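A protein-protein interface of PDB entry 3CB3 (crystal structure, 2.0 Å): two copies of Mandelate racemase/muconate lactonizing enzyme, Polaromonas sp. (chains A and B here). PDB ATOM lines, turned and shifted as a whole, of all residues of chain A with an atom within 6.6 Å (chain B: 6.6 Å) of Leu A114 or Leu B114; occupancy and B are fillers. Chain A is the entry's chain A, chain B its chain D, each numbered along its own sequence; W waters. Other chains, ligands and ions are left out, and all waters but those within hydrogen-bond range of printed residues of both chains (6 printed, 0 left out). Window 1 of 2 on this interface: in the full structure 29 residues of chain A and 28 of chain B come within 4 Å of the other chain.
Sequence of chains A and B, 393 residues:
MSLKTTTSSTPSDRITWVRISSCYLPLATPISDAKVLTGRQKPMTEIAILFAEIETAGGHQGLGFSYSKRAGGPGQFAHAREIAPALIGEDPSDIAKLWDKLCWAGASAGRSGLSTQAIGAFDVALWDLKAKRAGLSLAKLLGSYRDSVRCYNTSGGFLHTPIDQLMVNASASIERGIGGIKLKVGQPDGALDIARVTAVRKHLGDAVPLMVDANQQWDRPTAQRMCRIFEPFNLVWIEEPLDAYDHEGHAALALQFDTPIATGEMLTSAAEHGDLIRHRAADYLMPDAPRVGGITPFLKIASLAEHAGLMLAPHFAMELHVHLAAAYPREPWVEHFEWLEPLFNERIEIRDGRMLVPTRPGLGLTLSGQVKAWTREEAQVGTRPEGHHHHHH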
ATOM      1  N   SER A  68       4.933 -14.838  17.128  1.00  0.00           N
ATOM      2  CA  SER A  68       5.902 -15.579  16.330  1.00  0.00           C
ATOM      3  C   SER A  68       5.443 -17.031  16.353  1.00  0.00           C
ATOM      4  O   SER A  68       5.222 -17.590  17.422  1.00  0.00           O
ATOM      5  CB  SER A  68       7.304 -15.487  16.939  1.00  0.00           C
ATOM      6  OG  SER A  68       7.789 -14.158  16.953  1.00  0.00           O
ATOM      7  N   ALA A  71      10.552 -19.868  15.692  1.00  0.00           N
ATOM      8  CA  ALA A  71      11.497 -19.067  16.468  1.00  0.00           C
ATOM      9  C   ALA A  71      11.250 -17.578  16.218  1.00  0.00           C
ATOM     10  O   ALA A  71      10.853 -17.191  15.123  1.00  0.00           O
ATOM     11  CB  ALA A  71      12.937 -19.427  16.085  1.00  0.00           C
ATOM     12  N   GLY A  72      11.482 -16.751  17.233  1.00  0.00           N
ATOM     13  CA  GLY A  72      11.285 -15.319  17.069  1.00  0.00           C
ATOM     14  C   GLY A  72      10.698 -14.602  18.277  1.00  0.00           C
ATOM     15  O   GLY A  72      10.858 -13.387  18.415  1.00  0.00           O
ATOM     16  N   GLY A  73      10.022 -15.347  19.149  1.00  0.00           N
ATOM     17  CA  GLY A  73       9.419 -14.748  20.327  1.00  0.00           C
ATOM     18  C   GLY A  73      10.431 -14.054  21.221  1.00  0.00           C
ATOM     19  O   GLY A  73      10.257 -12.883  21.566  1.00  0.00           O
ATOM     20  N   GLY A  75      13.363 -12.992  20.535  1.00  0.00           N
ATOM     21  CA  GLY A  75      13.932 -11.859  19.825  1.00  0.00           C
ATOM     22  C   GLY A  75      13.000 -10.655  19.863  1.00  0.00           C
ATOM     23  O   GLY A  75      13.425  -9.542  20.178  1.00  0.00           O
ATOM     24  N   GLN A  76      11.729 -10.876  19.529  1.00  0.00           N
ATOM     25  CA  GLN A  76      10.732  -9.805  19.545  1.00  0.00           C
ATOM     26  C   GLN A  76      10.653  -9.127  20.911  1.00  0.00           C
ATOM     27  O   GLN A  76      10.706  -7.900  21.020  1.00  0.00           O
ATOM     28  CB  GLN A  76       9.353 -10.357  19.165  1.00  0.00           C
ATOM     29  CG  GLN A  76       9.114 -10.439  17.658  1.00  0.00           C
ATOM     30  CD  GLN A  76       7.759 -11.036  17.310  1.00  0.00           C
ATOM     31  OE1 GLN A  76       6.893 -11.177  18.170  1.00  0.00           O
ATOM     32  NE2 GLN A  76       7.570 -11.380  16.045  1.00  0.00           N
ATOM     33  N   HIS A  79      13.944  -7.088  21.801  1.00  0.00           N
ATOM     34  CA  HIS A  79      14.029  -5.800  21.119  1.00  0.00           C
ATOM     35  C   HIS A  79      12.997  -4.805  21.645  1.00  0.00           C
ATOM     36  O   HIS A  79      13.311  -3.634  21.880  1.00  0.00           O
ATOM     37  CB  HIS A  79      13.826  -5.978  19.617  1.00  0.00           C
ATOM     38  CG  HIS A  79      14.186  -4.766  18.818  1.00  0.00           C
ATOM     39  ND1 HIS A  79      15.477  -4.289  18.737  1.00  0.00           N
ATOM     40  CD2 HIS A  79      13.427  -3.929  18.073  1.00  0.00           C
ATOM     41  CE1 HIS A  79      15.497  -3.210  17.975  1.00  0.00           C
ATOM     42  NE2 HIS A  79      14.267  -2.971  17.558  1.00  0.00           N
ATOM     43  N   ALA A  80      11.763  -5.269  21.816  1.00  0.00           N
ATOM     44  CA  ALA A  80      10.693  -4.412  22.314  1.00  0.00           C
ATOM     45  C   ALA A  80      11.098  -3.806  23.650  1.00  0.00           C
ATOM     46  O   ALA A  80      10.845  -2.631  23.912  1.00  0.00           O
ATOM     47  CB  ALA A  80       9.413  -5.216  22.478  1.00  0.00           C
ATOM     48  N   GLY A 106      16.501   1.543  16.244  1.00  0.00           N
ATOM     49  CA  GLY A 106      17.159   0.294  15.899  1.00  0.00           C
ATOM     50  C   GLY A 106      17.340   0.273  14.397  1.00  0.00           C
ATOM     51  O   GLY A 106      17.101  -0.739  13.737  1.00  0.00           O
ATOM     52  N   SER A 108      19.816  -0.017  12.420  1.00  0.00           N
ATOM     53  CA  SER A 108      20.674  -1.031  11.807  1.00  0.00           C
ATOM     54  C   SER A 108      19.983  -2.394  11.756  1.00  0.00           C
ATOM     55  O   SER A 108      20.481  -3.329  11.130  1.00  0.00           O
ATOM     56  CB  SER A 108      22.002  -1.143  12.568  1.00  0.00           C
ATOM     57  OG  SER A 108      21.824  -1.669  13.872  1.00  0.00           O
ATOM     58  N   ALA A 109      18.834  -2.488  12.417  1.00  0.00           N
ATOM     59  CA  ALA A 109      18.049  -3.718  12.460  1.00  0.00           C
ATOM     60  C   ALA A 109      17.120  -3.832  11.254  1.00  0.00           C
ATOM     61  O   ALA A 109      16.481  -4.861  11.053  1.00  0.00           O
ATOM     62  CB  ALA A 109      17.238  -3.769  13.745  1.00  0.00           C
ATOM     63  N   GLY A 110      17.041  -2.769  10.461  1.00  0.00           N
ATOM     64  CA  GLY A 110      16.203  -2.789   9.277  1.00  0.00           C
ATOM     65  C   GLY A 110      14.766  -2.344   9.488  1.00  0.00           C
ATOM     66  O   GLY A 110      14.353  -2.038  10.602  1.00  0.00           O
ATOM     67  N   SER A 112      12.079  -4.256   8.719  1.00  0.00           N
ATOM     68  CA  SER A 112      11.302  -5.468   8.532  1.00  0.00           C
ATOM     69  C   SER A 112      11.813  -6.570   9.446  1.00  0.00           C
ATOM     70  O   SER A 112      12.930  -6.498   9.964  1.00  0.00           O
ATOM     71  CB  SER A 112      11.384  -5.935   7.080  1.00  0.00           C
ATOM     72  OG  SER A 112      12.709  -6.291   6.738  1.00  0.00           O
ATOM     73  N   GLY A 113      10.987  -7.587   9.642  1.00  0.00           N
ATOM     74  CA  GLY A 113      11.381  -8.694  10.489  1.00  0.00           C
ATOM     75  C   GLY A 113      11.103  -8.494  11.962  1.00  0.00           C
ATOM     76  O   GLY A 113      10.190  -7.761  12.352  1.00  0.00           O
ATOM     77  N   LEU A 114      11.914  -9.145  12.788  1.00  0.00           N
ATOM     78  CA  LEU A 114      11.755  -9.087  14.235  1.00  0.00           C
ATOM     79  C   LEU A 114      11.637  -7.699  14.863  1.00  0.00           C
ATOM     80  O   LEU A 114      10.810  -7.487  15.746  1.00  0.00           O
ATOM     81  CB  LEU A 114      12.901  -9.849  14.910  1.00  0.00           C
ATOM     82  CG  LEU A 114      12.895 -11.362  14.673  1.00  0.00           C
ATOM     83  CD1 LEU A 114      14.124 -12.007  15.334  1.00  0.00           C
ATOM     84  CD2 LEU A 114      11.614 -11.951  15.230  1.00  0.00           C
ATOM     85  N   SER A 115      12.462  -6.758  14.424  1.00  0.00           N
ATOM     86  CA  SER A 115      12.421  -5.428  15.014  1.00  0.00           C
ATOM     87  C   SER A 115      11.078  -4.743  14.791  1.00  0.00           C
ATOM     88  O   SER A 115      10.447  -4.275  15.746  1.00  0.00           O
ATOM     89  CB  SER A 115      13.570  -4.560  14.471  1.00  0.00           C
ATOM     90  OG  SER A 115      13.520  -4.433  13.056  1.00  0.00           O
ATOM     91  N   THR A 116      10.626  -4.693  13.543  1.00  0.00           N
ATOM     92  CA  THR A 116       9.358  -4.045  13.255  1.00  0.00           C
ATOM     93  C   THR A 116       8.155  -4.831  13.783  1.00  0.00           C
ATOM     94  O   THR A 116       7.085  -4.251  14.026  1.00  0.00           O
ATOM     95  CB  THR A 116       9.223  -3.728  11.740  1.00  0.00           C
ATOM     96  OG1 THR A 116       9.650  -4.854  10.966  1.00  0.00           O
ATOM     97  CG2 THR A 116      10.089  -2.523  11.377  1.00  0.00           C
ATOM     98  N   GLN A 117       8.318  -6.137  13.991  1.00  0.00           N
ATOM     99  CA  GLN A 117       7.218  -6.919  14.550  1.00  0.00           C
ATOM    100  C   GLN A 117       7.087  -6.537  16.022  1.00  0.00           C
ATOM    101  O   GLN A 117       5.990  -6.525  16.577  1.00  0.00           O
ATOM    102  CB  GLN A 117       7.464  -8.425  14.396  1.00  0.00           C
ATOM    103  CG  GLN A 117       7.320  -8.887  12.962  1.00  0.00           C
ATOM    104  CD  GLN A 117       7.732 -10.330  12.751  1.00  0.00           C
ATOM    105  OE1 GLN A 117       8.183 -11.016  13.678  1.00  0.00           O
ATOM    106  NE2 GLN A 117       7.583 -10.802  11.517  1.00  0.00           N
ATOM    107  N   ALA A 118       8.209  -6.207  16.653  1.00  0.00           N
ATOM    108  CA  ALA A 118       8.181  -5.788  18.049  1.00  0.00           C
ATOM    109  C   ALA A 118       7.509  -4.405  18.107  1.00  0.00           C
ATOM    110  O   ALA A 118       6.692  -4.123  18.993  1.00  0.00           O
ATOM    111  CB  ALA A 118       9.606  -5.717  18.607  1.00  0.00           C
ATOM    112  N   ILE A 119       7.858  -3.547  17.154  1.00  0.00           N
ATOM    113  CA  ILE A 119       7.281  -2.209  17.074  1.00  0.00           C
ATOM    114  C   ILE A 119       5.768  -2.344  16.852  1.00  0.00           C
ATOM    115  O   ILE A 119       4.968  -1.598  17.428  1.00  0.00           O
ATOM    116  CB  ILE A 119       7.901  -1.418  15.898  1.00  0.00           C
ATOM    117  CG1 ILE A 119       9.354  -1.060  16.228  1.00  0.00           C
ATOM    118  CG2 ILE A 119       7.092  -0.148  15.621  1.00  0.00           C
ATOM    119  CD1 ILE A 119      10.098  -0.398  15.073  1.00  0.00           C
ATOM    120  N   THR A 268       7.083  -9.716   5.573  1.00  0.00           N
ATOM    121  CA  THR A 268       7.225  -8.986   6.828  1.00  0.00           C
ATOM    122  C   THR A 268       7.411  -7.466   6.748  1.00  0.00           C
ATOM    123  O   THR A 268       7.988  -6.861   7.656  1.00  0.00           O
ATOM    124  CB  THR A 268       8.397  -9.566   7.655  1.00  0.00           C
ATOM    125  OG1 THR A 268       9.630  -9.307   6.974  1.00  0.00           O
ATOM    126  CG2 THR A 268       8.238 -11.089   7.823  1.00  0.00           C
ATOM    127  N   SER B  68      25.398  -4.631  16.420  1.00  0.00           N
ATOM    128  CA  SER B  68      24.324  -3.647  16.421  1.00  0.00           C
ATOM    129  C   SER B  68      24.898  -2.400  17.093  1.00  0.00           C
ATOM    130  O   SER B  68      25.386  -2.473  18.222  1.00  0.00           O
ATOM    131  CB  SER B  68      23.123  -4.146  17.230  1.00  0.00           C
ATOM    132  OG  SER B  68      22.624  -5.371  16.725  1.00  0.00           O
ATOM    133  N   ALA B  71      19.953   0.004  19.149  1.00  0.00           N
ATOM    134  CA  ALA B  71      19.139  -1.091  19.668  1.00  0.00           C
ATOM    135  C   ALA B  71      19.236  -2.297  18.733  1.00  0.00           C
ATOM    136  O   ALA B  71      19.389  -2.140  17.519  1.00  0.00           O
ATOM    137  CB  ALA B  71      17.694  -0.651  19.803  1.00  0.00           C
ATOM    138  N   GLY B  72      19.154  -3.498  19.301  1.00  0.00           N
ATOM    139  CA  GLY B  72      19.237  -4.701  18.486  1.00  0.00           C
ATOM    140  C   GLY B  72      20.122  -5.794  19.063  1.00  0.00           C
ATOM    141  O   GLY B  72      19.925  -6.974  18.772  1.00  0.00           O
ATOM    142  N   GLY B  73      21.095  -5.405  19.882  1.00  0.00           N
ATOM    143  CA  GLY B  73      21.995  -6.380  20.481  1.00  0.00           C
ATOM    144  C   GLY B  73      21.269  -7.509  21.188  1.00  0.00           C
ATOM    145  O   GLY B  73      21.493  -8.681  20.876  1.00  0.00           O
ATOM    146  N   PRO B  74      20.389  -7.190  22.150  1.00  0.00           N
ATOM    147  CA  PRO B  74      19.638  -8.213  22.887  1.00  0.00           C
ATOM    148  C   PRO B  74      18.756  -9.039  21.953  1.00  0.00           C
ATOM    149  O   PRO B  74      18.560 -10.237  22.163  1.00  0.00           O
ATOM    150  CB  PRO B  74      18.819  -7.391  23.884  1.00  0.00           C
ATOM    151  CG  PRO B  74      19.684  -6.162  24.103  1.00  0.00           C
ATOM    152  CD  PRO B  74      20.128  -5.846  22.700  1.00  0.00           C
ATOM    153  N   GLY B  75      18.230  -8.388  20.921  1.00  0.00           N
ATOM    154  CA  GLY B  75      17.380  -9.075  19.964  1.00  0.00           C
ATOM    155  C   GLY B  75      18.163 -10.114  19.183  1.00  0.00           C
ATOM    156  O   GLY B  75      17.739 -11.264  19.077  1.00  0.00           O
ATOM    157  N   GLN B  76      19.307  -9.718  18.632  1.00  0.00           N
ATOM    158  CA  GLN B  76      20.126 -10.660  17.877  1.00  0.00           C
ATOM    159  C   GLN B  76      20.496 -11.856  18.752  1.00  0.00           C
ATOM    160  O   GLN B  76      20.382 -13.010  18.329  1.00  0.00           O
ATOM    161  CB  GLN B  76      21.412  -9.993  17.384  1.00  0.00           C
ATOM    162  CG  GLN B  76      21.221  -8.845  16.414  1.00  0.00           C
ATOM    163  CD  GLN B  76      22.549  -8.250  15.995  1.00  0.00           C
ATOM    164  OE1 GLN B  76      23.519  -8.317  16.743  1.00  0.00           O
ATOM    165  NE2 GLN B  76      22.598  -7.658  14.808  1.00  0.00           N
ATOM    166  N   HIS B  79      17.503 -14.324  19.579  1.00  0.00           N
ATOM    167  CA  HIS B  79      17.115 -15.127  18.428  1.00  0.00           C
ATOM    168  C   HIS B  79      18.190 -16.159  18.125  1.00  0.00           C
ATOM    169  O   HIS B  79      17.883 -17.313  17.819  1.00  0.00           O
ATOM    170  CB  HIS B  79      16.903 -14.256  17.193  1.00  0.00           C
ATOM    171  CG  HIS B  79      16.295 -14.997  16.043  1.00  0.00           C
ATOM    172  ND1 HIS B  79      15.005 -15.482  16.073  1.00  0.00           N
ATOM    173  CD2 HIS B  79      16.806 -15.355  14.841  1.00  0.00           C
ATOM    174  CE1 HIS B  79      14.748 -16.105  14.936  1.00  0.00           C
ATOM    175  NE2 HIS B  79      15.823 -16.042  14.172  1.00  0.00           N
ATOM    176  N   ALA B  80      19.447 -15.735  18.210  1.00  0.00           N
ATOM    177  CA  ALA B  80      20.582 -16.617  17.952  1.00  0.00           C
ATOM    178  C   ALA B  80      20.555 -17.801  18.909  1.00  0.00           C
ATOM    179  O   ALA B  80      20.817 -18.933  18.519  1.00  0.00           O
ATOM    180  CB  ALA B  80      21.895 -15.850  18.121  1.00  0.00           C
ATOM    181  N   SER B 108       8.530 -17.031  10.358  1.00  0.00           N
ATOM    182  CA  SER B 108       7.698 -15.829  10.440  1.00  0.00           C
ATOM    183  C   SER B 108       8.522 -14.602  10.795  1.00  0.00           C
ATOM    184  O   SER B 108       8.000 -13.492  10.847  1.00  0.00           O
ATOM    185  CB  SER B 108       6.595 -16.006  11.488  1.00  0.00           C
ATOM    186  OG  SER B 108       7.126 -15.971  12.805  1.00  0.00           O
ATOM    187  N   ALA B 109       9.810 -14.812  11.033  1.00  0.00           N
ATOM    188  CA  ALA B 109      10.714 -13.731  11.401  1.00  0.00           C
ATOM    189  C   ALA B 109      11.277 -12.949  10.216  1.00  0.00           C
ATOM    190  O   ALA B 109      11.917 -11.918  10.410  1.00  0.00           O
ATOM    191  CB  ALA B 109      11.859 -14.283  12.255  1.00  0.00           C
ATOM    192  N   GLY B 110      11.051 -13.432   8.998  1.00  0.00           N
ATOM    193  CA  GLY B 110      11.542 -12.726   7.824  1.00  0.00           C
ATOM    194  C   GLY B 110      12.919 -13.136   7.323  1.00  0.00           C
ATOM    195  O   GLY B 110      13.642 -13.877   7.993  1.00  0.00           O
ATOM    196  N   SER B 112      15.282 -10.893   6.617  1.00  0.00           N
ATOM    197  CA  SER B 112      16.091  -9.695   6.794  1.00  0.00           C
ATOM    198  C   SER B 112      15.943  -9.191   8.216  1.00  0.00           C
ATOM    199  O   SER B 112      15.098  -9.669   8.967  1.00  0.00           O
ATOM    200  CB  SER B 112      15.635  -8.597   5.818  1.00  0.00           C
ATOM    201  OG  SER B 112      14.262  -8.275   6.016  1.00  0.00           O
ATOM    202  N   GLY B 113      16.764  -8.218   8.584  1.00  0.00           N
ATOM    203  CA  GLY B 113      16.682  -7.674   9.923  1.00  0.00           C
ATOM    204  C   GLY B 113      17.409  -8.504  10.962  1.00  0.00           C
ATOM    205  O   GLY B 113      18.365  -9.228  10.651  1.00  0.00           O
ATOM    206  N   LEU B 114      16.944  -8.396  12.201  1.00  0.00           N
ATOM    207  CA  LEU B 114      17.547  -9.084  13.332  1.00  0.00           C
ATOM    208  C   LEU B 114      17.723 -10.595  13.210  1.00  0.00           C
ATOM    209  O   LEU B 114      18.738 -11.137  13.653  1.00  0.00           O
ATOM    210  CB  LEU B 114      16.745  -8.802  14.604  1.00  0.00           C
ATOM    211  CG  LEU B 114      16.706  -7.369  15.127  1.00  0.00           C
ATOM    212  CD1 LEU B 114      15.824  -7.316  16.374  1.00  0.00           C
ATOM    213  CD2 LEU B 114      18.111  -6.891  15.436  1.00  0.00           C
ATOM    214  N   SER B 115      16.740 -11.278  12.632  1.00  0.00           N
ATOM    215  CA  SER B 115      16.830 -12.728  12.520  1.00  0.00           C
ATOM    216  C   SER B 115      17.992 -13.168  11.640  1.00  0.00           C
ATOM    217  O   SER B 115      18.759 -14.050  12.023  1.00  0.00           O
ATOM    218  CB  SER B 115      15.508 -13.317  12.001  1.00  0.00           C
ATOM    219  OG  SER B 115      15.213 -12.867  10.689  1.00  0.00           O
ATOM    220  N   THR B 116      18.140 -12.554  10.472  1.00  0.00           N
ATOM    221  CA  THR B 116      19.225 -12.936   9.587  1.00  0.00           C
ATOM    222  C   THR B 116      20.580 -12.406  10.064  1.00  0.00           C
ATOM    223  O   THR B 116      21.620 -12.982   9.750  1.00  0.00           O
ATOM    224  CB  THR B 116      18.942 -12.494   8.130  1.00  0.00           C
ATOM    225  OG1 THR B 116      18.484 -11.139   8.118  1.00  0.00           O
ATOM    226  CG2 THR B 116      17.857 -13.385   7.509  1.00  0.00           C
ATOM    227  N   GLN B 117      20.578 -11.322  10.832  1.00  0.00           N
ATOM    228  CA  GLN B 117      21.841 -10.793  11.348  1.00  0.00           C
ATOM    229  C   GLN B 117      22.364 -11.790  12.390  1.00  0.00           C
ATOM    230  O   GLN B 117      23.571 -12.028  12.486  1.00  0.00           O
ATOM    231  CB  GLN B 117      21.639  -9.398  11.958  1.00  0.00           C
ATOM    232  CG  GLN B 117      21.353  -8.337  10.893  1.00  0.00           C
ATOM    233  CD  GLN B 117      20.937  -6.987  11.463  1.00  0.00           C
ATOM    234  OE1 GLN B 117      20.746  -6.832  12.669  1.00  0.00           O
ATOM    235  NE2 GLN B 117      20.784  -6.008  10.588  1.00  0.00           N
ATOM    236  N   ALA B 118      21.452 -12.384  13.157  1.00  0.00           N
ATOM    237  CA  ALA B 118      21.840 -13.390  14.145  1.00  0.00           C
ATOM    238  C   ALA B 118      22.376 -14.596  13.368  1.00  0.00           C
ATOM    239  O   ALA B 118      23.376 -15.201  13.746  1.00  0.00           O
ATOM    240  CB  ALA B 118      20.641 -13.802  14.989  1.00  0.00           C
ATOM    241  N   ILE B 119      21.692 -14.940  12.282  1.00  0.00           N
ATOM    242  CA  ILE B 119      22.111 -16.044  11.426  1.00  0.00           C
ATOM    243  C   ILE B 119      23.519 -15.749  10.885  1.00  0.00           C
ATOM    244  O   ILE B 119      24.360 -16.646  10.792  1.00  0.00           O
ATOM    245  CB  ILE B 119      21.121 -16.228  10.235  1.00  0.00           C
ATOM    246  CG1 ILE B 119      19.799 -16.814  10.743  1.00  0.00           C
ATOM    247  CG2 ILE B 119      21.716 -17.139   9.184  1.00  0.00           C
ATOM    248  CD1 ILE B 119      18.772 -17.097   9.644  1.00  0.00           C
ATOM    249  N   THR B 268      19.576  -4.343   4.891  1.00  0.00           N
ATOM    250  CA  THR B 268      19.770  -5.564   5.672  1.00  0.00           C
ATOM    251  C   THR B 268      19.441  -6.888   4.981  1.00  0.00           C
ATOM    252  O   THR B 268      19.110  -7.868   5.649  1.00  0.00           O
ATOM    253  CB  THR B 268      18.954  -5.497   6.978  1.00  0.00           C
ATOM    254  OG1 THR B 268      17.561  -5.410   6.659  1.00  0.00           O
ATOM    255  CG2 THR B 268      19.346  -4.262   7.802  1.00  0.00           C
HETATM  256  O   HOH W   1      14.300 -10.270  11.415  1.00  0.00           O
HETATM  257  O   HOH W   2      13.770 -15.298  18.921  1.00  0.00           O
HETATM  258  O   HOH W   3      21.820  -4.486  13.949  1.00  0.00           O
HETATM  259  O   HOH W   4      11.884 -10.503   5.157  1.00  0.00           O
HETATM  260  O   HOH W   5      14.403  -6.834  12.192  1.00  0.00           O
HETATM  261  O   HOH W   6      17.278  -5.738  20.605  1.00  0.00           O
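Water W1 lies within hydrogen-bond range of the backbone carbonyl oxygen (O) of Ser B112, the side-chain hydroxyl (OG) of Ser B115, the backbone NH (N) of Leu A114, the backbone carbonyl oxygen (O) of Ala B109 and the backbone NH (N) of Leu B114. Water W5 lies within hydrogen-bond range of O of Ser A112 (2.7 Å), OG of Ser A115 (2.7 Å), N of Leu B114 (3.0 Å), O of Ala A109 (3.1 Å) and N of Leu A114 (3.4 Å). Water W3 lies within hydrogen-bond range of the side-chain hydroxyl (OG) of Ser A108 (2.8 Å), the side-chain amide oxygen (OE1) of Gln B117 (2.9 Å), the side-chain hydroxyl (OG) of Ser B68 (3.0 Å) and the side-chain amide nitrogen (NE2) of Gln B76 (3.4 Å). Water W6 lies within hydrogen-bond range of N of Gly B75 (2.8 Å), ND1 of His A79 (3.0 Å) and N of Gly B72 (3.2 Å). Water W2 lies within hydrogen-bond range of N of Gly A75, ND1 of His B79 and N of Gly A72. Water W4 bridges OG1 of Thr A268 (3.1 Å) and OG of Ser B112 (3.4 Å).
Of the 21 printed residues of chain B, 13 touch a printed residue of chain A. Of the 21 printed residues of chain A, 15 touch a printed residue of chain B. Among the printed residues, no Asp or Glu carboxylate lies within 4 Å of a Lys or Arg side-chain nitrogen of the other chain.
OG of Ser B112 sits at hydrogen-bond distance from OG of Ser A112 (2.6 Å). The side-chain amide nitrogen of Gln A117 lies within hydrogen-bond range of the backbone carbonyl oxygen of Ser B108 (2.8 Å). The backbone carbonyl oxygen (O) of Ser A108 sits at hydrogen-bond distance from the side-chain amide nitrogen (NE2) of Gln B117 (2.8 Å).
Among the printed residues, pairs that only touch across the chains: Ala A109 with Gly B113 (3.0 Å), Gly A113 with Ala B109 (3.3 Å), Ser A108 with Thr B268 (3.6 Å), Leu A114 with Ala B109 (3.7 Å), Ala A109 with Leu B114 (3.7 Å), Leu A114 with His B79 (3.7 Å), Gly A106 with Ala B71 (3.7 Å), Thr A268 with Gly B110 (3.7 Å), Ser A68 with Ser B108 (3.8 Å), Gly A110 with Thr B268 (3.8 Å), His A79 with Gly B72 (3.8 Å), Leu A114 with Ser B115 (3.8 Å), His A79 with Ala B71 (3.8 Å), Gly A72 with His B79 (3.9 Å), His A79 with Leu B114 (3.9 Å), Thr A268 with Ser B108 (3.9 Å), Gly A75 with Gly B75 (3.9 Å), Ser A115 with Leu B114 (3.9 Å), Ser A112 with Gly B113 (3.9 Å), Ala A71 with His B79 (3.95 Å) and Leu A114 with Leu B114 (3.996 Å).
Of the printed residues of chain A, Leu B114 touches His A79, Ala A109, Leu A114 and Ser A115. Printed residues of chain B within 4 Å of Ala A109: Gly B113 and Leu B114. Of the printed residues of chain A, Ser B112 touches Ser A112 (2.6 Å). Of the printed residues of chain A, Gly B113 touches Ala A109 and Ser A112. Printed residues of chain A within 4 Å of Gly B72: His A79 (3.8 Å). Ala B80 touches none of the printed residues of chain A.
Ser A68 touches Ser B108, but with the chains exchanged Ser A108 does not touch Ser B68 (4.1 Å). Gly A72 touches His B79, and with the chains exchanged His A79 touches Gly B72. Ser A108 touches Gln B117, and with the chains exchanged Gln A117 touches Ser B108. Leu A114 touches Ser B115, and with the chains exchanged Ser A115 touches Leu B114. Positions printed for both chains: 68, 71, 72, 73, 75, 76, 79, 80, 108, 109, 110, 112, 113, 114, 115, 116, 117, 118, 119 and 268. Of the 24 pairs that touch across the chains among the printed residues, 21 have their exchanged pair printed and touching as well.
The backbone NH (N) of Ser A112 lies close to the side-chain hydroxyl (OG1) of Thr A116 (3.4 Å). NE2 of Gln B76 sits at hydrogen-bond distance from OE1 of Gln B117. The side-chain hydroxyl (OG1) of Thr B116 is in hydrogen-bond range of the backbone carbonyl oxygen (O) of Gly B113, 3.2 Å away. The side-chain hydroxyl (OG1) of Thr A116 is in hydrogen-bond range of the backbone carbonyl oxygen (O) of Gly A113 (3.3 Å). N of Gly A73 sits at hydrogen-bond distance from OG of Ser A68, at 3.3 Å. O of Gly B110 lies within hydrogen-bond range of OG of Ser B115, at 3.3 Å.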
